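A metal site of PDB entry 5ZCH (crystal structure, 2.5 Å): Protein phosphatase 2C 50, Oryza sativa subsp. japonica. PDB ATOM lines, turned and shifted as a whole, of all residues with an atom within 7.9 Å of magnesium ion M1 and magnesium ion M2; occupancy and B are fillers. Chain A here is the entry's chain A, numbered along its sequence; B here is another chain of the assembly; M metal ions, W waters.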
ATOM      1  N   SER A  13      11.882  12.746 -26.579  1.00  0.00           N
ATOM      2  CA  SER A  13      10.873  13.709 -26.982  1.00  0.00           C
ATOM      3  C   SER A  13      11.500  15.113 -27.054  1.00  0.00           C
ATOM      4  O   SER A  13      12.575  15.367 -26.508  1.00  0.00           O
ATOM      5  CB  SER A  13       9.688  13.697 -26.020  1.00  0.00           C
ATOM      6  OG  SER A  13       8.785  12.662 -26.347  1.00  0.00           O
ATOM      7  N   GLU A  15      10.423  18.123 -25.922  1.00  0.00           N
ATOM      8  CA  GLU A  15      10.445  18.879 -24.676  1.00  0.00           C
ATOM      9  C   GLU A  15       9.736  18.072 -23.583  1.00  0.00           C
ATOM     10  O   GLU A  15       9.166  17.009 -23.832  1.00  0.00           O
ATOM     11  CB  GLU A  15       9.837  20.274 -24.846  1.00  0.00           C
ATOM     12  CG  GLU A  15       8.516  20.329 -25.567  1.00  0.00           C
ATOM     13  CD  GLU A  15       8.376  21.585 -26.410  1.00  0.00           C
ATOM     14  OE1 GLU A  15       7.619  21.570 -27.404  1.00  0.00           O
ATOM     15  OE2 GLU A  15       9.043  22.594 -26.084  1.00  0.00           O
ATOM     16  N   MET A  16       9.757  18.620 -22.374  1.00  0.00           N
ATOM     17  CA  MET A  16       9.378  17.916 -21.167  1.00  0.00           C
ATOM     18  C   MET A  16       8.023  18.433 -20.670  1.00  0.00           C
ATOM     19  O   MET A  16       7.899  19.597 -20.305  1.00  0.00           O
ATOM     20  CB  MET A  16      10.435  18.090 -20.072  1.00  0.00           C
ATOM     21  CG  MET A  16      10.120  17.370 -18.775  1.00  0.00           C
ATOM     22  SD  MET A  16       9.714  15.628 -19.015  1.00  0.00           S
ATOM     23  CE  MET A  16      10.231  14.944 -17.448  1.00  0.00           C
ATOM     24  N   GLU A  17       7.022  17.553 -20.671  1.00  0.00           N
ATOM     25  CA  GLU A  17       5.682  17.894 -20.210  1.00  0.00           C
ATOM     26  C   GLU A  17       5.233  17.005 -19.058  1.00  0.00           C
ATOM     27  O   GLU A  17       4.077  17.116 -18.619  1.00  0.00           O
ATOM     28  CB  GLU A  17       4.688  17.816 -21.367  1.00  0.00           C
ATOM     29  CG  GLU A  17       5.003  18.785 -22.498  1.00  0.00           C
ATOM     30  CD  GLU A  17       4.045  18.660 -23.673  1.00  0.00           C
ATOM     31  OE1 GLU A  17       3.379  17.606 -23.784  1.00  0.00           O
ATOM     32  OE2 GLU A  17       3.971  19.606 -24.489  1.00  0.00           O
ATOM     33  N   ASP A  18       6.107  16.142 -18.557  1.00  0.00           N
ATOM     34  CA  ASP A  18       5.814  15.384 -17.350  1.00  0.00           C
ATOM     35  C   ASP A  18       6.140  16.209 -16.111  1.00  0.00           C
ATOM     36  O   ASP A  18       6.983  17.109 -16.142  1.00  0.00           O
ATOM     37  CB  ASP A  18       6.623  14.083 -17.330  1.00  0.00           C
ATOM     38  CG  ASP A  18       5.894  12.922 -17.987  1.00  0.00           C
ATOM     39  OD1 ASP A  18       4.938  13.186 -18.745  1.00  0.00           O
ATOM     40  OD2 ASP A  18       6.284  11.760 -17.741  1.00  0.00           O
ATOM     41  N   ALA A  19       5.459  15.896 -15.007  1.00  0.00           N
ATOM     42  CA  ALA A  19       5.723  16.540 -13.734  1.00  0.00           C
ATOM     43  C   ALA A  19       5.496  15.537 -12.616  1.00  0.00           C
ATOM     44  O   ALA A  19       4.713  14.592 -12.763  1.00  0.00           O
ATOM     45  CB  ALA A  19       4.853  17.782 -13.531  1.00  0.00           C
ATOM     46  N   PHE A  60       2.242  13.488 -13.003  1.00  0.00           N
ATOM     47  CA  PHE A  60       1.336  14.268 -13.835  1.00  0.00           C
ATOM     48  C   PHE A  60       1.884  14.330 -15.253  1.00  0.00           C
ATOM     49  O   PHE A  60       2.876  15.021 -15.512  1.00  0.00           O
ATOM     50  CB  PHE A  60       1.128  15.667 -13.247  1.00  0.00           C
ATOM     51  CG  PHE A  60       0.917  15.676 -11.763  1.00  0.00           C
ATOM     52  CD1 PHE A  60      -0.312  15.310 -11.228  1.00  0.00           C
ATOM     53  CD2 PHE A  60       1.938  16.023 -10.896  1.00  0.00           C
ATOM     54  CE1 PHE A  60      -0.509  15.316  -9.861  1.00  0.00           C
ATOM     55  CE2 PHE A  60       1.745  16.022  -9.534  1.00  0.00           C
ATOM     56  CZ  PHE A  60       0.517  15.676  -9.011  1.00  0.00           C
ATOM     57  N   ASP A  61       1.238  13.606 -16.172  1.00  0.00           N
ATOM     58  CA  ASP A  61       1.641  13.538 -17.569  1.00  0.00           C
ATOM     59  C   ASP A  61       0.814  14.549 -18.351  1.00  0.00           C
ATOM     60  O   ASP A  61      -0.363  14.311 -18.642  1.00  0.00           O
ATOM     61  CB  ASP A  61       1.470  12.122 -18.111  1.00  0.00           C
ATOM     62  CG  ASP A  61       2.096  11.936 -19.489  1.00  0.00           C
ATOM     63  OD1 ASP A  61       2.457  12.936 -20.137  1.00  0.00           O
ATOM     64  OD2 ASP A  61       2.231  10.772 -19.912  1.00  0.00           O
ATOM     65  N   GLY A  62       1.428  15.687 -18.705  1.00  0.00           N
ATOM     66  CA  GLY A  62       0.721  16.706 -19.432  1.00  0.00           C
ATOM     67  C   GLY A  62       0.697  16.462 -20.931  1.00  0.00           C
ATOM     68  O   GLY A  62       1.495  15.715 -21.491  1.00  0.00           O
ATOM     69  N   HIS A  63      -0.257  17.119 -21.593  1.00  0.00           N
ATOM     70  CA  HIS A  63      -0.365  17.069 -23.043  1.00  0.00           C
ATOM     71  C   HIS A  63      -0.847  18.425 -23.540  1.00  0.00           C
ATOM     72  O   HIS A  63      -1.575  19.145 -22.841  1.00  0.00           O
ATOM     73  CB  HIS A  63      -1.320  15.964 -23.501  1.00  0.00           C
ATOM     74  CG  HIS A  63      -2.665  15.998 -22.840  1.00  0.00           C
ATOM     75  ND1 HIS A  63      -3.025  15.116 -21.839  1.00  0.00           N
ATOM     76  CD2 HIS A  63      -3.734  16.817 -23.024  1.00  0.00           C
ATOM     77  CE1 HIS A  63      -4.254  15.381 -21.449  1.00  0.00           C
ATOM     78  NE2 HIS A  63      -4.703  16.408 -22.143  1.00  0.00           N
ATOM     79  N   GLY A  64      -0.424  18.776 -24.756  1.00  0.00           N
ATOM     80  CA  GLY A  64      -0.688  20.108 -25.269  1.00  0.00           C
ATOM     81  C   GLY A  64       0.124  21.201 -24.616  1.00  0.00           C
ATOM     82  O   GLY A  64      -0.139  22.381 -24.860  1.00  0.00           O
ATOM     83  N   GLY A  65       1.111  20.837 -23.809  1.00  0.00           N
ATOM     84  CA  GLY A  65       1.881  21.796 -23.027  1.00  0.00           C
ATOM     85  C   GLY A  65       2.206  21.216 -21.671  1.00  0.00           C
ATOM     86  O   GLY A  65       1.671  20.162 -21.298  1.00  0.00           O
ATOM     87  N   ALA A  66       3.062  21.890 -20.911  1.00  0.00           N
ATOM     88  CA  ALA A  66       3.472  21.407 -19.599  1.00  0.00           C
ATOM     89  C   ALA A  66       2.834  22.186 -18.448  1.00  0.00           C
ATOM     90  O   ALA A  66       3.101  21.865 -17.289  1.00  0.00           O
ATOM     91  CB  ALA A  66       4.999  21.443 -19.467  1.00  0.00           C
ATOM     92  N   ALA A  69       0.294  20.204 -16.111  1.00  0.00           N
ATOM     93  CA  ALA A  69       1.049  19.240 -15.303  1.00  0.00           C
ATOM     94  C   ALA A  69       1.859  19.952 -14.226  1.00  0.00           C
ATOM     95  O   ALA A  69       1.933  19.484 -13.087  1.00  0.00           O
ATOM     96  CB  ALA A  69       1.949  18.395 -16.198  1.00  0.00           C
ATOM     97  N   GLY A 143      -3.935  19.773 -21.090  1.00  0.00           N
ATOM     98  CA  GLY A 143      -4.396  18.969 -19.986  1.00  0.00           C
ATOM     99  C   GLY A 143      -3.275  18.174 -19.345  1.00  0.00           C
ATOM    100  O   GLY A 143      -2.103  18.389 -19.667  1.00  0.00           O
ATOM    101  N   SER A 144      -3.611  17.249 -18.447  1.00  0.00           N
ATOM    102  CA  SER A 144      -2.609  16.441 -17.785  1.00  0.00           C
ATOM    103  C   SER A 144      -3.283  15.282 -17.068  1.00  0.00           C
ATOM    104  O   SER A 144      -4.383  15.433 -16.535  1.00  0.00           O
ATOM    105  CB  SER A 144      -1.781  17.268 -16.783  1.00  0.00           C
ATOM    106  OG  SER A 144      -0.904  16.438 -16.046  1.00  0.00           O
ATOM    107  N   THR A 145      -2.612  14.130 -17.062  1.00  0.00           N
ATOM    108  CA  THR A 145      -3.017  13.040 -16.187  1.00  0.00           C
ATOM    109  C   THR A 145      -2.690  13.377 -14.739  1.00  0.00           C
ATOM    110  O   THR A 145      -1.950  14.314 -14.441  1.00  0.00           O
ATOM    111  CB  THR A 145      -2.338  11.734 -16.597  1.00  0.00           C
ATOM    112  OG1 THR A 145      -1.030  11.682 -16.007  1.00  0.00           O
ATOM    113  CG2 THR A 145      -2.213  11.632 -18.113  1.00  0.00           C
ATOM    114  N   ASP A 163      -4.088   8.023 -18.057  1.00  0.00           N
ATOM    115  CA  ASP A 163      -3.426   6.769 -18.418  1.00  0.00           C
ATOM    116  C   ASP A 163      -2.087   6.597 -17.720  1.00  0.00           C
ATOM    117  O   ASP A 163      -1.255   5.786 -18.159  1.00  0.00           O
ATOM    118  CB  ASP A 163      -3.265   6.666 -19.942  1.00  0.00           C
ATOM    119  CG  ASP A 163      -2.414   7.790 -20.514  1.00  0.00           C
ATOM    120  OD1 ASP A 163      -2.048   8.717 -19.775  1.00  0.00           O
ATOM    121  OD2 ASP A 163      -2.124   7.737 -21.733  1.00  0.00           O
ATOM    122  N   SER A 164      -1.843   7.346 -16.651  1.00  0.00           N
ATOM    123  CA  SER A 164      -0.754   7.023 -15.750  1.00  0.00           C
ATOM    124  C   SER A 164      -1.199   5.922 -14.804  1.00  0.00           C
ATOM    125  O   SER A 164      -2.391   5.682 -14.612  1.00  0.00           O
ATOM    126  CB  SER A 164      -0.304   8.256 -14.974  1.00  0.00           C
ATOM    127  OG  SER A 164       0.208   9.255 -15.835  1.00  0.00           O
ATOM    128  N   MET A 213      -7.076   9.452 -23.965  1.00  0.00           N
ATOM    129  CA  MET A 213      -7.555   9.097 -22.636  1.00  0.00           C
ATOM    130  C   MET A 213      -8.926   9.731 -22.430  1.00  0.00           C
ATOM    131  O   MET A 213      -9.280  10.708 -23.078  1.00  0.00           O
ATOM    132  CB  MET A 213      -6.580   9.546 -21.546  1.00  0.00           C
ATOM    133  CG  MET A 213      -6.564  11.041 -21.291  1.00  0.00           C
ATOM    134  SD  MET A 213      -5.053  11.578 -20.464  1.00  0.00           S
ATOM    135  CE  MET A 213      -3.812  10.989 -21.615  1.00  0.00           C
ATOM    136  N   SER A 248       4.279   7.579 -15.393  1.00  0.00           N
ATOM    137  CA  SER A 248       3.506   7.952 -16.570  1.00  0.00           C
ATOM    138  C   SER A 248       3.555   6.832 -17.601  1.00  0.00           C
ATOM    139  O   SER A 248       4.275   5.839 -17.447  1.00  0.00           O
ATOM    140  CB  SER A 248       4.032   9.255 -17.166  1.00  0.00           C
ATOM    141  OG  SER A 248       5.439   9.205 -17.357  1.00  0.00           O
ATOM    142  N   ASP A 249       2.779   7.000 -18.666  1.00  0.00           N
ATOM    143  CA  ASP A 249       2.722   5.970 -19.712  1.00  0.00           C
ATOM    144  C   ASP A 249       4.054   5.792 -20.423  1.00  0.00           C
ATOM    145  O   ASP A 249       4.213   4.799 -21.144  1.00  0.00           O
ATOM    146  CB  ASP A 249       1.620   6.297 -20.721  1.00  0.00           C
ATOM    147  CG  ASP A 249       1.836   7.629 -21.422  1.00  0.00           C
ATOM    148  OD1 ASP A 249       2.854   8.305 -21.158  1.00  0.00           O
ATOM    149  OD2 ASP A 249       0.975   8.011 -22.250  1.00  0.00           O
ATOM    150  N   GLY A 250       5.017   6.697 -20.234  1.00  0.00           N
ATOM    151  CA  GLY A 250       6.331   6.509 -20.811  1.00  0.00           C
ATOM    152  C   GLY A 250       7.002   5.225 -20.349  1.00  0.00           C
ATOM    153  O   GLY A 250       7.847   4.666 -21.060  1.00  0.00           O
ATOM    154  N   LEU A 251       6.638   4.744 -19.159  1.00  0.00           N
ATOM    155  CA  LEU A 251       7.143   3.472 -18.653  1.00  0.00           C
ATOM    156  C   LEU A 251       6.206   2.311 -18.995  1.00  0.00           C
ATOM    157  O   LEU A 251       6.657   1.278 -19.500  1.00  0.00           O
ATOM    158  CB  LEU A 251       7.359   3.551 -17.149  1.00  0.00           C
ATOM    159  CG  LEU A 251       7.821   2.250 -16.478  1.00  0.00           C
ATOM    160  CD1 LEU A 251       9.345   2.187 -16.423  1.00  0.00           C
ATOM    161  CD2 LEU A 251       7.229   2.103 -15.088  1.00  0.00           C
ATOM    162  N   ASP A 253       4.123   1.910 -21.328  1.00  0.00           N
ATOM    163  CA  ASP A 253       3.938   1.604 -22.739  1.00  0.00           C
ATOM    164  C   ASP A 253       4.906   0.541 -23.231  1.00  0.00           C
ATOM    165  O   ASP A 253       4.644  -0.091 -24.255  1.00  0.00           O
ATOM    166  CB  ASP A 253       4.079   2.865 -23.588  1.00  0.00           C
ATOM    167  CG  ASP A 253       2.817   3.701 -23.609  1.00  0.00           C
ATOM    168  OD1 ASP A 253       1.730   3.142 -23.381  1.00  0.00           O
ATOM    169  OD2 ASP A 253       2.919   4.922 -23.864  1.00  0.00           O
ATOM    170  N   ASP A 311       8.976   8.670 -25.351  1.00  0.00           N
ATOM    171  CA  ASP A 311       8.186   9.630 -24.598  1.00  0.00           C
ATOM    172  C   ASP A 311       8.939  10.066 -23.339  1.00  0.00           C
ATOM    173  O   ASP A 311       9.964   9.494 -22.958  1.00  0.00           O
ATOM    174  CB  ASP A 311       6.834   9.034 -24.226  1.00  0.00           C
ATOM    175  CG  ASP A 311       5.800  10.091 -23.854  1.00  0.00           C
ATOM    176  OD1 ASP A 311       6.096  11.290 -24.041  1.00  0.00           O
ATOM    177  OD2 ASP A 311       4.714   9.715 -23.367  1.00  0.00           O
ATOM    178  N   ASN A 312       8.437  11.128 -22.709  1.00  0.00           N
ATOM    179  CA  ASN A 312       8.922  11.510 -21.390  1.00  0.00           C
ATOM    180  C   ASN A 312       8.738  10.347 -20.420  1.00  0.00           C
ATOM    181  O   ASN A 312       7.747   9.616 -20.492  1.00  0.00           O
ATOM    182  CB  ASN A 312       8.170  12.741 -20.873  1.00  0.00           C
ATOM    183  CG  ASN A 312       8.296  13.928 -21.808  1.00  0.00           C
ATOM    184  OD1 ASN A 312       7.436  14.799 -21.839  1.00  0.00           O
ATOM    185  ND2 ASN A 312       9.384  13.969 -22.578  1.00  0.00           N
ATOM    186  N   ILE A 313       9.696  10.182 -19.519  1.00  0.00           N
ATOM    187  CA  ILE A 313       9.665   9.112 -18.520  1.00  0.00           C
ATOM    188  C   ILE A 313       9.728   9.749 -17.136  1.00  0.00           C
ATOM    189  O   ILE A 313      10.622  10.571 -16.868  1.00  0.00           O
ATOM    190  CB  ILE A 313      10.820   8.121 -18.711  1.00  0.00           C
ATOM    191  CG1 ILE A 313      11.061   7.848 -20.195  1.00  0.00           C
ATOM    192  CG2 ILE A 313      10.539   6.824 -17.957  1.00  0.00           C
ATOM    193  CD1 ILE A 313       9.986   7.030 -20.845  1.00  0.00           C
ATOM    194  N   SER B  71       1.578  18.169 -28.460  1.00  0.00           N
ATOM    195  CA  SER B  71       1.336  16.786 -28.099  1.00  0.00           C
ATOM    196  C   SER B  71      -0.134  16.553 -27.761  1.00  0.00           C
ATOM    197  O   SER B  71      -0.929  17.490 -27.644  1.00  0.00           O
ATOM    198  CB  SER B  71       2.217  16.381 -26.917  1.00  0.00           C
ATOM    199  OG  SER B  71       1.901  17.132 -25.764  1.00  0.00           O
ATOM    200  N   GLY B  72      -0.491  15.280 -27.616  1.00  0.00           N
ATOM    201  CA  GLY B  72      -1.860  14.883 -27.318  1.00  0.00           C
ATOM    202  C   GLY B  72      -2.733  14.646 -28.529  1.00  0.00           C
ATOM    203  O   GLY B  72      -3.868  14.177 -28.373  1.00  0.00           O
HETATM  204 MG    MG M   1       3.057  10.226 -21.808  1.00  0.00          MG
HETATM  205 MG    MG M   2       3.081  14.077 -21.765  1.00  0.00          MG
HETATM  206  O   HOH W   1       1.429  10.333 -23.117  1.00  0.00           O
HETATM  207  O   HOH W   2       1.228  13.069 -23.034  1.00  0.00           O
HETATM  208  O   HOH W   3       3.721  12.057 -22.706  1.00  0.00           O
HETATM  209  O   HOH W   4       5.047  10.418 -20.518  1.00  0.00           O
HETATM  210  O   HOH W   5       3.252  14.804 -23.909  1.00  0.00           O
HETATM  211  O   HOH W   6       5.042  14.481 -21.191  1.00  0.00           O
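The side-chain carboxylate of Asp 18 is in hydrogen-bond range of the side-chain hydroxyl of Ser 248 (2.7 Å).
OG of Ser 144 lies close to O of Asp 61, at 3.4 Å.
The backbone NH (N) of Asp 18 sits close to the side-chain sulfur (SD) of Met 16.
O of Asp 61 is in hydrogen-bond range of N of Thr 145, 2.8 Å away.
N of Gly 62 is in hydrogen-bond range of O of Glu 17 (3.0 Å).
The nearest printed residue that does not touch magnesium ion M1 is Gly 250 (4.3 Å).
Asp 18 touches magnesium ion M2.
Of the 30 residues printed, 3 come within 4 Å of magnesium ion M2.
Magnesium ion M1 is bound by the side-chain carboxylate of Asp 249 (2.0 Å), water W1 (2.1 Å), the side-chain carboxylate of Asp 61 (2.1 Å), water W3 (2.1 Å), the side-chain carboxylate of Asp 311 (2.3 Å) and water W4 (2.4 Å).
Magnesium ion M2 is bound by water W6 (2.1 Å), the side-chain carboxylate of Asp 61 (2.1 Å), water W5 (2.3 Å), the backbone carbonyl oxygen of Gly 62 (2.3 Å), water W3 (2.3 Å) and water W2 (2.5 Å).
Magnesium ion M2 has six donor atoms within binding distance.
Water W4 lies within hydrogen-bond range of O of Asn 312 (2.8 Å), OD1 of Asp 18 (3.3 Å) and OG of Ser 248 (3.4 Å).
Water W5 bridges the side-chain carboxylate of Glu 17 (2.8 Å) and the side-chain hydroxyl of Ser 71 of chain B (3.3 Å).
Water W6 lies within hydrogen-bond range of OD1 of Asn 312 (2.5 Å) and OD1 of Asp 18 (2.8 Å).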
